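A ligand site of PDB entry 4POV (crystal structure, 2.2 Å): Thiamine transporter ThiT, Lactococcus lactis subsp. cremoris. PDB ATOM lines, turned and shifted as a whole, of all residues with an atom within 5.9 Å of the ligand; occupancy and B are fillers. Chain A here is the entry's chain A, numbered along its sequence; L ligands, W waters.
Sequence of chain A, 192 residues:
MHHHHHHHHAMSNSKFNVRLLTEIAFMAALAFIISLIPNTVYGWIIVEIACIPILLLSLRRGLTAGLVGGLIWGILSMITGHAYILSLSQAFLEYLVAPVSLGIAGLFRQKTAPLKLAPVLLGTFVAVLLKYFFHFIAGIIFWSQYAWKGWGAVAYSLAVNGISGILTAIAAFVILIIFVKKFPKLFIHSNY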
ATOM      1  N   TRP A  44       4.489   7.504   1.902  1.00  0.00           N
ATOM      2  CA  TRP A  44       5.668   6.690   2.273  1.00  0.00           C
ATOM      3  C   TRP A  44       5.486   5.226   1.877  1.00  0.00           C
ATOM      4  O   TRP A  44       6.289   4.370   2.235  1.00  0.00           O
ATOM      5  CB  TRP A  44       5.964   6.817   3.774  1.00  0.00           C
ATOM      6  CG  TRP A  44       7.048   7.814   4.063  1.00  0.00           C
ATOM      7  CD1 TRP A  44       6.904   9.049   4.663  1.00  0.00           C
ATOM      8  CD2 TRP A  44       8.432   7.687   3.751  1.00  0.00           C
ATOM      9  NE1 TRP A  44       8.127   9.678   4.735  1.00  0.00           N
ATOM     10  CE2 TRP A  44       9.077   8.857   4.190  1.00  0.00           C
ATOM     11  CE3 TRP A  44       9.209   6.670   3.150  1.00  0.00           C
ATOM     12  CZ2 TRP A  44      10.453   9.051   4.040  1.00  0.00           C
ATOM     13  CZ3 TRP A  44      10.561   6.860   3.008  1.00  0.00           C
ATOM     14  CH2 TRP A  44      11.180   8.047   3.443  1.00  0.00           C
ATOM     15  N   ILE A  46       6.191   2.825  -0.796  1.00  0.00           N
ATOM     16  CA  ILE A  46       7.221   2.898  -1.827  1.00  0.00           C
ATOM     17  C   ILE A  46       7.527   1.485  -2.321  1.00  0.00           C
ATOM     18  O   ILE A  46       7.220   0.492  -1.619  1.00  0.00           O
ATOM     19  CB  ILE A  46       8.523   3.560  -1.307  1.00  0.00           C
ATOM     20  CG1 ILE A  46       9.098   2.762  -0.129  1.00  0.00           C
ATOM     21  CG2 ILE A  46       8.283   5.039  -0.901  1.00  0.00           C
ATOM     22  CD1 ILE A  46      10.494   3.219   0.221  1.00  0.00           C
ATOM     23  N   GLU A  48      10.882  -0.324  -2.990  1.00  0.00           N
ATOM     24  CA  GLU A  48      12.328  -0.060  -2.845  1.00  0.00           C
ATOM     25  C   GLU A  48      13.235  -0.968  -3.692  1.00  0.00           C
ATOM     26  O   GLU A  48      13.950  -1.805  -3.152  1.00  0.00           O
ATOM     27  CB  GLU A  48      12.754  -0.143  -1.380  1.00  0.00           C
ATOM     28  CG  GLU A  48      14.153   0.510  -1.121  1.00  0.00           C
ATOM     29  CD  GLU A  48      14.487   0.653   0.372  1.00  0.00           C
ATOM     30  OE1 GLU A  48      13.963  -0.154   1.172  1.00  0.00           O
ATOM     31  OE2 GLU A  48      15.248   1.571   0.735  1.00  0.00           O
ATOM     32  N   TYR A  84      15.937  10.550   4.806  1.00  0.00           N
ATOM     33  CA  TYR A  84      14.977  11.353   5.563  1.00  0.00           C
ATOM     34  C   TYR A  84      15.259  11.066   7.025  1.00  0.00           C
ATOM     35  O   TYR A  84      15.003   9.958   7.527  1.00  0.00           O
ATOM     36  CB  TYR A  84      13.535  11.005   5.151  1.00  0.00           C
ATOM     37  CG  TYR A  84      13.260  11.378   3.715  1.00  0.00           C
ATOM     38  CD1 TYR A  84      13.523  10.487   2.684  1.00  0.00           C
ATOM     39  CD2 TYR A  84      12.756  12.627   3.383  1.00  0.00           C
ATOM     40  CE1 TYR A  84      13.274  10.854   1.341  1.00  0.00           C
ATOM     41  CE2 TYR A  84      12.505  12.995   2.060  1.00  0.00           C
ATOM     42  CZ  TYR A  84      12.780  12.104   1.051  1.00  0.00           C
ATOM     43  OH  TYR A  84      12.526  12.458  -0.262  1.00  0.00           O
ATOM     44  N   GLN A  90      16.656   7.497  15.012  1.00  0.00           N
ATOM     45  CA  GLN A  90      15.796   7.091  13.896  1.00  0.00           C
ATOM     46  C   GLN A  90      16.639   6.835  12.654  1.00  0.00           C
ATOM     47  O   GLN A  90      16.332   5.937  11.870  1.00  0.00           O
ATOM     48  CB  GLN A  90      14.717   8.160  13.600  1.00  0.00           C
ATOM     49  CG  GLN A  90      13.959   7.960  12.270  1.00  0.00           C
ATOM     50  CD  GLN A  90      14.661   8.600  11.083  1.00  0.00           C
ATOM     51  OE1 GLN A  90      15.462   9.512  11.260  1.00  0.00           O
ATOM     52  NE2 GLN A  90      14.373   8.108   9.866  1.00  0.00           N
ATOM     53  N   GLU A  94      16.871   3.360  10.681  1.00  0.00           N
ATOM     54  CA  GLU A  94      16.300   3.201   9.317  1.00  0.00           C
ATOM     55  C   GLU A  94      17.310   3.258   8.184  1.00  0.00           C
ATOM     56  O   GLU A  94      17.013   2.836   7.062  1.00  0.00           O
ATOM     57  CB  GLU A  94      15.208   4.252   9.061  1.00  0.00           C
ATOM     58  CG  GLU A  94      14.063   4.226  10.069  1.00  0.00           C
ATOM     59  CD  GLU A  94      12.765   4.772   9.459  1.00  0.00           C
ATOM     60  OE1 GLU A  94      12.112   4.017   8.715  1.00  0.00           O
ATOM     61  OE2 GLU A  94      12.418   5.964   9.689  1.00  0.00           O
ATOM     62  N   TYR A  95      18.483   3.824   8.456  1.00  0.00           N
ATOM     63  CA  TYR A  95      19.534   3.982   7.461  1.00  0.00           C
ATOM     64  C   TYR A  95      20.850   3.287   7.810  1.00  0.00           C
ATOM     65  O   TYR A  95      21.773   3.290   6.983  1.00  0.00           O
ATOM     66  CB  TYR A  95      19.785   5.482   7.229  1.00  0.00           C
ATOM     67  CG  TYR A  95      18.647   6.108   6.459  1.00  0.00           C
ATOM     68  CD1 TYR A  95      18.548   5.935   5.081  1.00  0.00           C
ATOM     69  CD2 TYR A  95      17.670   6.859   7.117  1.00  0.00           C
ATOM     70  CE1 TYR A  95      17.503   6.489   4.375  1.00  0.00           C
ATOM     71  CE2 TYR A  95      16.624   7.414   6.420  1.00  0.00           C
ATOM     72  CZ  TYR A  95      16.538   7.240   5.053  1.00  0.00           C
ATOM     73  OH  TYR A  95      15.503   7.829   4.366  1.00  0.00           O
ATOM     74  N   LYS A 131      13.950  -6.014   6.870  1.00  0.00           N
ATOM     75  CA  LYS A 131      14.126  -4.598   6.645  1.00  0.00           C
ATOM     76  C   LYS A 131      12.801  -3.841   7.007  1.00  0.00           C
ATOM     77  O   LYS A 131      12.839  -2.857   7.719  1.00  0.00           O
ATOM     78  CB  LYS A 131      14.517  -4.289   5.206  1.00  0.00           C
ATOM     79  CG  LYS A 131      14.935  -2.843   5.023  1.00  0.00           C
ATOM     80  CD  LYS A 131      15.510  -2.575   3.634  1.00  0.00           C
ATOM     81  CE  LYS A 131      16.292  -1.258   3.594  1.00  0.00           C
ATOM     82  NZ  LYS A 131      15.472  -0.023   3.404  1.00  0.00           N
ATOM     83  N   TYR A 132      11.638  -4.310   6.529  1.00  0.00           N
ATOM     84  CA  TYR A 132      10.444  -3.444   6.646  1.00  0.00           C
ATOM     85  C   TYR A 132       9.828  -3.657   8.017  1.00  0.00           C
ATOM     86  O   TYR A 132       9.077  -2.826   8.511  1.00  0.00           O
ATOM     87  CB  TYR A 132       9.498  -3.643   5.469  1.00  0.00           C
ATOM     88  CG  TYR A 132       9.899  -2.648   4.404  1.00  0.00           C
ATOM     89  CD1 TYR A 132      10.931  -2.939   3.514  1.00  0.00           C
ATOM     90  CD2 TYR A 132       9.341  -1.351   4.377  1.00  0.00           C
ATOM     91  CE1 TYR A 132      11.373  -1.972   2.576  1.00  0.00           C
ATOM     92  CE2 TYR A 132       9.773  -0.389   3.458  1.00  0.00           C
ATOM     93  CZ  TYR A 132      10.796  -0.715   2.549  1.00  0.00           C
ATOM     94  OH  TYR A 132      11.233   0.225   1.632  1.00  0.00           O
ATOM     95  N   PHE A 134      11.868  -3.302  10.609  1.00  0.00           N
ATOM     96  CA  PHE A 134      12.503  -2.149  11.269  1.00  0.00           C
ATOM     97  C   PHE A 134      11.856  -0.810  10.828  1.00  0.00           C
ATOM     98  O   PHE A 134      11.662   0.071  11.664  1.00  0.00           O
ATOM     99  CB  PHE A 134      14.012  -2.132  11.011  1.00  0.00           C
ATOM    100  CG  PHE A 134      14.758  -3.288  11.663  1.00  0.00           C
ATOM    101  CD1 PHE A 134      14.720  -3.456  13.027  1.00  0.00           C
ATOM    102  CD2 PHE A 134      15.494  -4.164  10.918  1.00  0.00           C
ATOM    103  CE1 PHE A 134      15.396  -4.471  13.613  1.00  0.00           C
ATOM    104  CE2 PHE A 134      16.142  -5.190  11.493  1.00  0.00           C
ATOM    105  CZ  PHE A 134      16.106  -5.345  12.846  1.00  0.00           C
ATOM    106  N   HIS A 135      11.464  -0.672   9.574  1.00  0.00           N
ATOM    107  CA  HIS A 135      10.748   0.557   9.193  1.00  0.00           C
ATOM    108  C   HIS A 135       9.399   0.664   9.912  1.00  0.00           C
ATOM    109  O   HIS A 135       8.985   1.766  10.343  1.00  0.00           O
ATOM    110  CB  HIS A 135      10.568   0.623   7.683  1.00  0.00           C
ATOM    111  CG  HIS A 135      11.863   0.715   6.947  1.00  0.00           C
ATOM    112  ND1 HIS A 135      12.761   1.744   7.146  1.00  0.00           N
ATOM    113  CD2 HIS A 135      12.430  -0.114   6.023  1.00  0.00           C
ATOM    114  CE1 HIS A 135      13.816   1.562   6.353  1.00  0.00           C
ATOM    115  NE2 HIS A 135      13.636   0.433   5.676  1.00  0.00           N
ATOM    116  N   PHE A 136       8.767  -0.485  10.128  1.00  0.00           N
ATOM    117  CA  PHE A 136       7.471  -0.587  10.794  1.00  0.00           C
ATOM    118  C   PHE A 136       7.574  -0.134  12.237  1.00  0.00           C
ATOM    119  O   PHE A 136       6.747   0.664  12.735  1.00  0.00           O
ATOM    120  CB  PHE A 136       6.916  -2.022  10.712  1.00  0.00           C
ATOM    121  CG  PHE A 136       5.814  -2.324  11.709  1.00  0.00           C
ATOM    122  CD1 PHE A 136       4.540  -1.760  11.564  1.00  0.00           C
ATOM    123  CD2 PHE A 136       6.049  -3.171  12.797  1.00  0.00           C
ATOM    124  CE1 PHE A 136       3.532  -2.013  12.467  1.00  0.00           C
ATOM    125  CE2 PHE A 136       5.037  -3.437  13.720  1.00  0.00           C
ATOM    126  CZ  PHE A 136       3.762  -2.853  13.544  1.00  0.00           C
ATOM    127  N   ALA A 138      10.048   1.769  13.293  1.00  0.00           N
ATOM    128  CA  ALA A 138      10.322   3.214  13.196  1.00  0.00           C
ATOM    129  C   ALA A 138       9.041   4.003  12.957  1.00  0.00           C
ATOM    130  O   ALA A 138       8.926   5.109  13.476  1.00  0.00           O
ATOM    131  CB  ALA A 138      11.300   3.518  12.086  1.00  0.00           C
ATOM    132  N   GLY A 139       8.107   3.442  12.164  1.00  0.00           N
ATOM    133  CA  GLY A 139       6.897   4.137  11.766  1.00  0.00           C
ATOM    134  C   GLY A 139       6.091   4.425  13.030  1.00  0.00           C
ATOM    135  O   GLY A 139       5.599   5.542  13.261  1.00  0.00           O
ATOM    136  N   ILE A 140       6.060   3.443  13.919  1.00  0.00           N
ATOM    137  CA  ILE A 140       5.440   3.625  15.207  1.00  0.00           C
ATOM    138  C   ILE A 140       6.119   4.695  16.036  1.00  0.00           C
ATOM    139  O   ILE A 140       5.448   5.515  16.639  1.00  0.00           O
ATOM    140  CB  ILE A 140       5.412   2.355  16.021  1.00  0.00           C
ATOM    141  CG1 ILE A 140       4.667   1.267  15.257  1.00  0.00           C
ATOM    142  CG2 ILE A 140       4.689   2.630  17.365  1.00  0.00           C
ATOM    143  CD1 ILE A 140       4.587  -0.045  15.978  1.00  0.00           C
ATOM    144  N   TRP A 143       7.146   8.373  13.228  1.00  0.00           N
ATOM    145  CA  TRP A 143       6.352   8.894  12.135  1.00  0.00           C
ATOM    146  C   TRP A 143       4.848   8.964  12.439  1.00  0.00           C
ATOM    147  O   TRP A 143       4.052   9.202  11.543  1.00  0.00           O
ATOM    148  CB  TRP A 143       6.604   8.031  10.901  1.00  0.00           C
ATOM    149  CG  TRP A 143       8.056   8.037  10.417  1.00  0.00           C
ATOM    150  CD1 TRP A 143       9.065   7.180  10.795  1.00  0.00           C
ATOM    151  CD2 TRP A 143       8.628   8.923   9.456  1.00  0.00           C
ATOM    152  NE1 TRP A 143      10.222   7.505  10.134  1.00  0.00           N
ATOM    153  CE2 TRP A 143       9.983   8.564   9.305  1.00  0.00           C
ATOM    154  CE3 TRP A 143       8.112  10.005   8.710  1.00  0.00           C
ATOM    155  CZ2 TRP A 143      10.833   9.223   8.444  1.00  0.00           C
ATOM    156  CZ3 TRP A 143       8.962  10.678   7.868  1.00  0.00           C
ATOM    157  CH2 TRP A 143      10.319  10.284   7.730  1.00  0.00           C
ATOM    158  N   TYR A 156      -1.394   2.369  11.277  1.00  0.00           N
ATOM    159  CA  TYR A 156      -0.820   3.209  10.238  1.00  0.00           C
ATOM    160  C   TYR A 156       0.588   2.708   9.779  1.00  0.00           C
ATOM    161  O   TYR A 156       0.865   2.599   8.564  1.00  0.00           O
ATOM    162  CB  TYR A 156      -0.751   4.649  10.736  1.00  0.00           C
ATOM    163  CG  TYR A 156       0.006   5.573   9.820  1.00  0.00           C
ATOM    164  CD1 TYR A 156      -0.460   5.840   8.532  1.00  0.00           C
ATOM    165  CD2 TYR A 156       1.158   6.205  10.238  1.00  0.00           C
ATOM    166  CE1 TYR A 156       0.224   6.705   7.704  1.00  0.00           C
ATOM    167  CE2 TYR A 156       1.847   7.062   9.420  1.00  0.00           C
ATOM    168  CZ  TYR A 156       1.384   7.308   8.144  1.00  0.00           C
ATOM    169  OH  TYR A 156       2.079   8.158   7.327  1.00  0.00           O
ATOM    170  N   SER A 157       1.478   2.397  10.718  1.00  0.00           N
ATOM    171  CA  SER A 157       2.812   1.936  10.320  1.00  0.00           C
ATOM    172  C   SER A 157       2.701   0.578   9.632  1.00  0.00           C
ATOM    173  O   SER A 157       3.313   0.358   8.587  1.00  0.00           O
ATOM    174  CB  SER A 157       3.782   1.848  11.505  1.00  0.00           C
ATOM    175  OG  SER A 157       5.082   1.579  11.013  1.00  0.00           O
ATOM    176  N   VAL A 160       1.440   1.154   6.046  1.00  0.00           N
ATOM    177  CA  VAL A 160       2.397   1.807   5.185  1.00  0.00           C
ATOM    178  C   VAL A 160       3.608   0.912   4.951  1.00  0.00           C
ATOM    179  O   VAL A 160       4.112   0.786   3.809  1.00  0.00           O
ATOM    180  CB  VAL A 160       2.911   3.148   5.762  1.00  0.00           C
ATOM    181  CG1 VAL A 160       4.103   3.614   4.985  1.00  0.00           C
ATOM    182  CG2 VAL A 160       1.794   4.233   5.723  1.00  0.00           C
ATOM    183  N   ASN A 161       4.135   0.358   6.030  1.00  0.00           N
ATOM    184  CA  ASN A 161       5.364  -0.421   5.881  1.00  0.00           C
ATOM    185  C   ASN A 161       5.068  -1.887   5.474  1.00  0.00           C
ATOM    186  O   ASN A 161       5.880  -2.507   4.763  1.00  0.00           O
ATOM    187  CB  ASN A 161       6.162  -0.300   7.149  1.00  0.00           C
ATOM    188  CG  ASN A 161       6.636   1.115   7.365  1.00  0.00           C
ATOM    189  OD1 ASN A 161       7.312   1.672   6.493  1.00  0.00           O
ATOM    190  ND2 ASN A 161       6.280   1.715   8.494  1.00  0.00           N
ATOM    191  N   SER A 164       4.548  -1.310   1.647  1.00  0.00           N
ATOM    192  CA  SER A 164       5.864  -1.093   1.057  1.00  0.00           C
ATOM    193  C   SER A 164       6.722  -2.379   1.033  1.00  0.00           C
ATOM    194  O   SER A 164       7.356  -2.677   0.044  1.00  0.00           O
ATOM    195  CB  SER A 164       6.632  -0.017   1.795  1.00  0.00           C
ATOM    196  OG  SER A 164       6.065   1.258   1.546  1.00  0.00           O
HETATM  197  C1  LIG L   1       4.841   5.498   8.501  1.00  0.00           C
HETATM  198  N1  LIG L   1       9.387   3.858   8.672  1.00  0.00           N
HETATM  199  C2  LIG L   1      13.107   5.737   5.744  1.00  0.00           C
HETATM  200  O1  LIG L   1      14.318   4.066   3.813  1.00  0.00           O
HETATM  201  C3  LIG L   1      13.237   3.241   3.544  1.00  0.00           C
HETATM  202  C4  LIG L   1       9.727   4.045   5.373  1.00  0.00           C
HETATM  203  S1  LIG L   1      10.565   3.082   4.241  1.00  0.00           S
HETATM  204  C5  LIG L   1      12.066   3.759   4.368  1.00  0.00           C
HETATM  205  C6  LIG L   1      11.976   4.839   5.314  1.00  0.00           C
HETATM  206  C7  LIG L   1      10.658   5.013   5.871  1.00  0.00           C
HETATM  207  C8  LIG L   1      10.335   6.075   6.906  1.00  0.00           C
HETATM  208  C9  LIG L   1       8.487   4.826   8.197  1.00  0.00           C
HETATM  209  N2  LIG L   1       7.184   4.739   8.529  1.00  0.00           N
HETATM  210  C10 LIG L   1       6.308   5.642   8.091  1.00  0.00           C
HETATM  211  N3  LIG L   1       6.662   6.662   7.312  1.00  0.00           N
HETATM  212  C11 LIG L   1       7.924   6.837   6.911  1.00  0.00           C
HETATM  213  C12 LIG L   1       8.902   5.901   7.361  1.00  0.00           C
HETATM  214  O   HOH W   1       4.757   8.795   7.589  1.00  0.00           O
HETATM  215  O   HOH W   2      17.112   2.489   4.264  1.00  0.00           O
HETATM  216  O   HOH W   3       7.381   2.319   3.826  1.00  0.00           O
HETATM  217  O   HOH W   4      14.969   6.471   1.665  1.00  0.00           O
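CG of Trp 44 touches C11 of the ligand, at 3.1 Å. Glu 48 touches the ligand. Tyr 95 touches the ligand (OH to C2, 3.5 Å). Lys 131 touches the ligand. Tyr 132 touches the ligand. Ala 138 touches the ligand (CB to N1, 3.9 Å). Gly 139 touches the ligand (CA to N2, 3.3 Å). CD2 of Trp 143 touches C11 of the ligand, 3.4 Å away. Tyr 156 touches the ligand (CE2 to C1, 3.5 Å). The nearest printed residue that does not touch the ligand is Ile 46 (4.02 Å).
Water W1 lies within hydrogen-bond range of OH of Tyr 156 and N3 of the ligand. Water W2 lies within hydrogen-bond range of O of Glu 94 (2.8 Å), NZ of Lys 131 (3.1 Å) and O1 of the ligand (3.2 Å). Water W4 bridges OH of Tyr 95 (3.1 Å) and O1 of the ligand (3.3 Å).
A ring nitrogen (ND1) of His 135 sits at hydrogen-bond distance from the side-chain carboxylate (OE1) of Glu 94, at 2.8 Å. The side-chain carboxylate (OE2) of Glu 94 is in hydrogen-bond range of the indole nitrogen (NE1) of Trp 143, 2.7 Å away. The side-chain amide nitrogen of Gln 90 lies within hydrogen-bond range of the side-chain carboxylate of Glu 94 (2.9 Å). O of Trp 44 lies within hydrogen-bond range of OG of Ser 164 (3.2 Å). The side-chain amide nitrogen of Asn 161 sits at hydrogen-bond distance from the side-chain hydroxyl of Ser 157, 2.8 Å away. The side-chain hydroxyl (OH) of Tyr 95 lies within hydrogen-bond range of the backbone NH (N) of Tyr 84, at 2.8 Å. OH of Tyr 132 lies within hydrogen-bond range of OE1 of Glu 48 (2.8 Å). The side-chain carboxylate (OE1) of Glu 48 lies within salt-bridge range of the side-chain amino group (NZ) of Lys 131 (2.7 Å).
N1 of the ligand is in hydrogen-bond range of O of His 135 (2.7 Å). The side-chain carboxylate (OE1) of Glu 94 sits at hydrogen-bond distance from a nitrogen (N1) of the ligand (2.7 Å). The side-chain amide nitrogen (ND2) of Asn 161 lies within hydrogen-bond range of a nitrogen (N2) of the ligand, 3.2 Å away.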
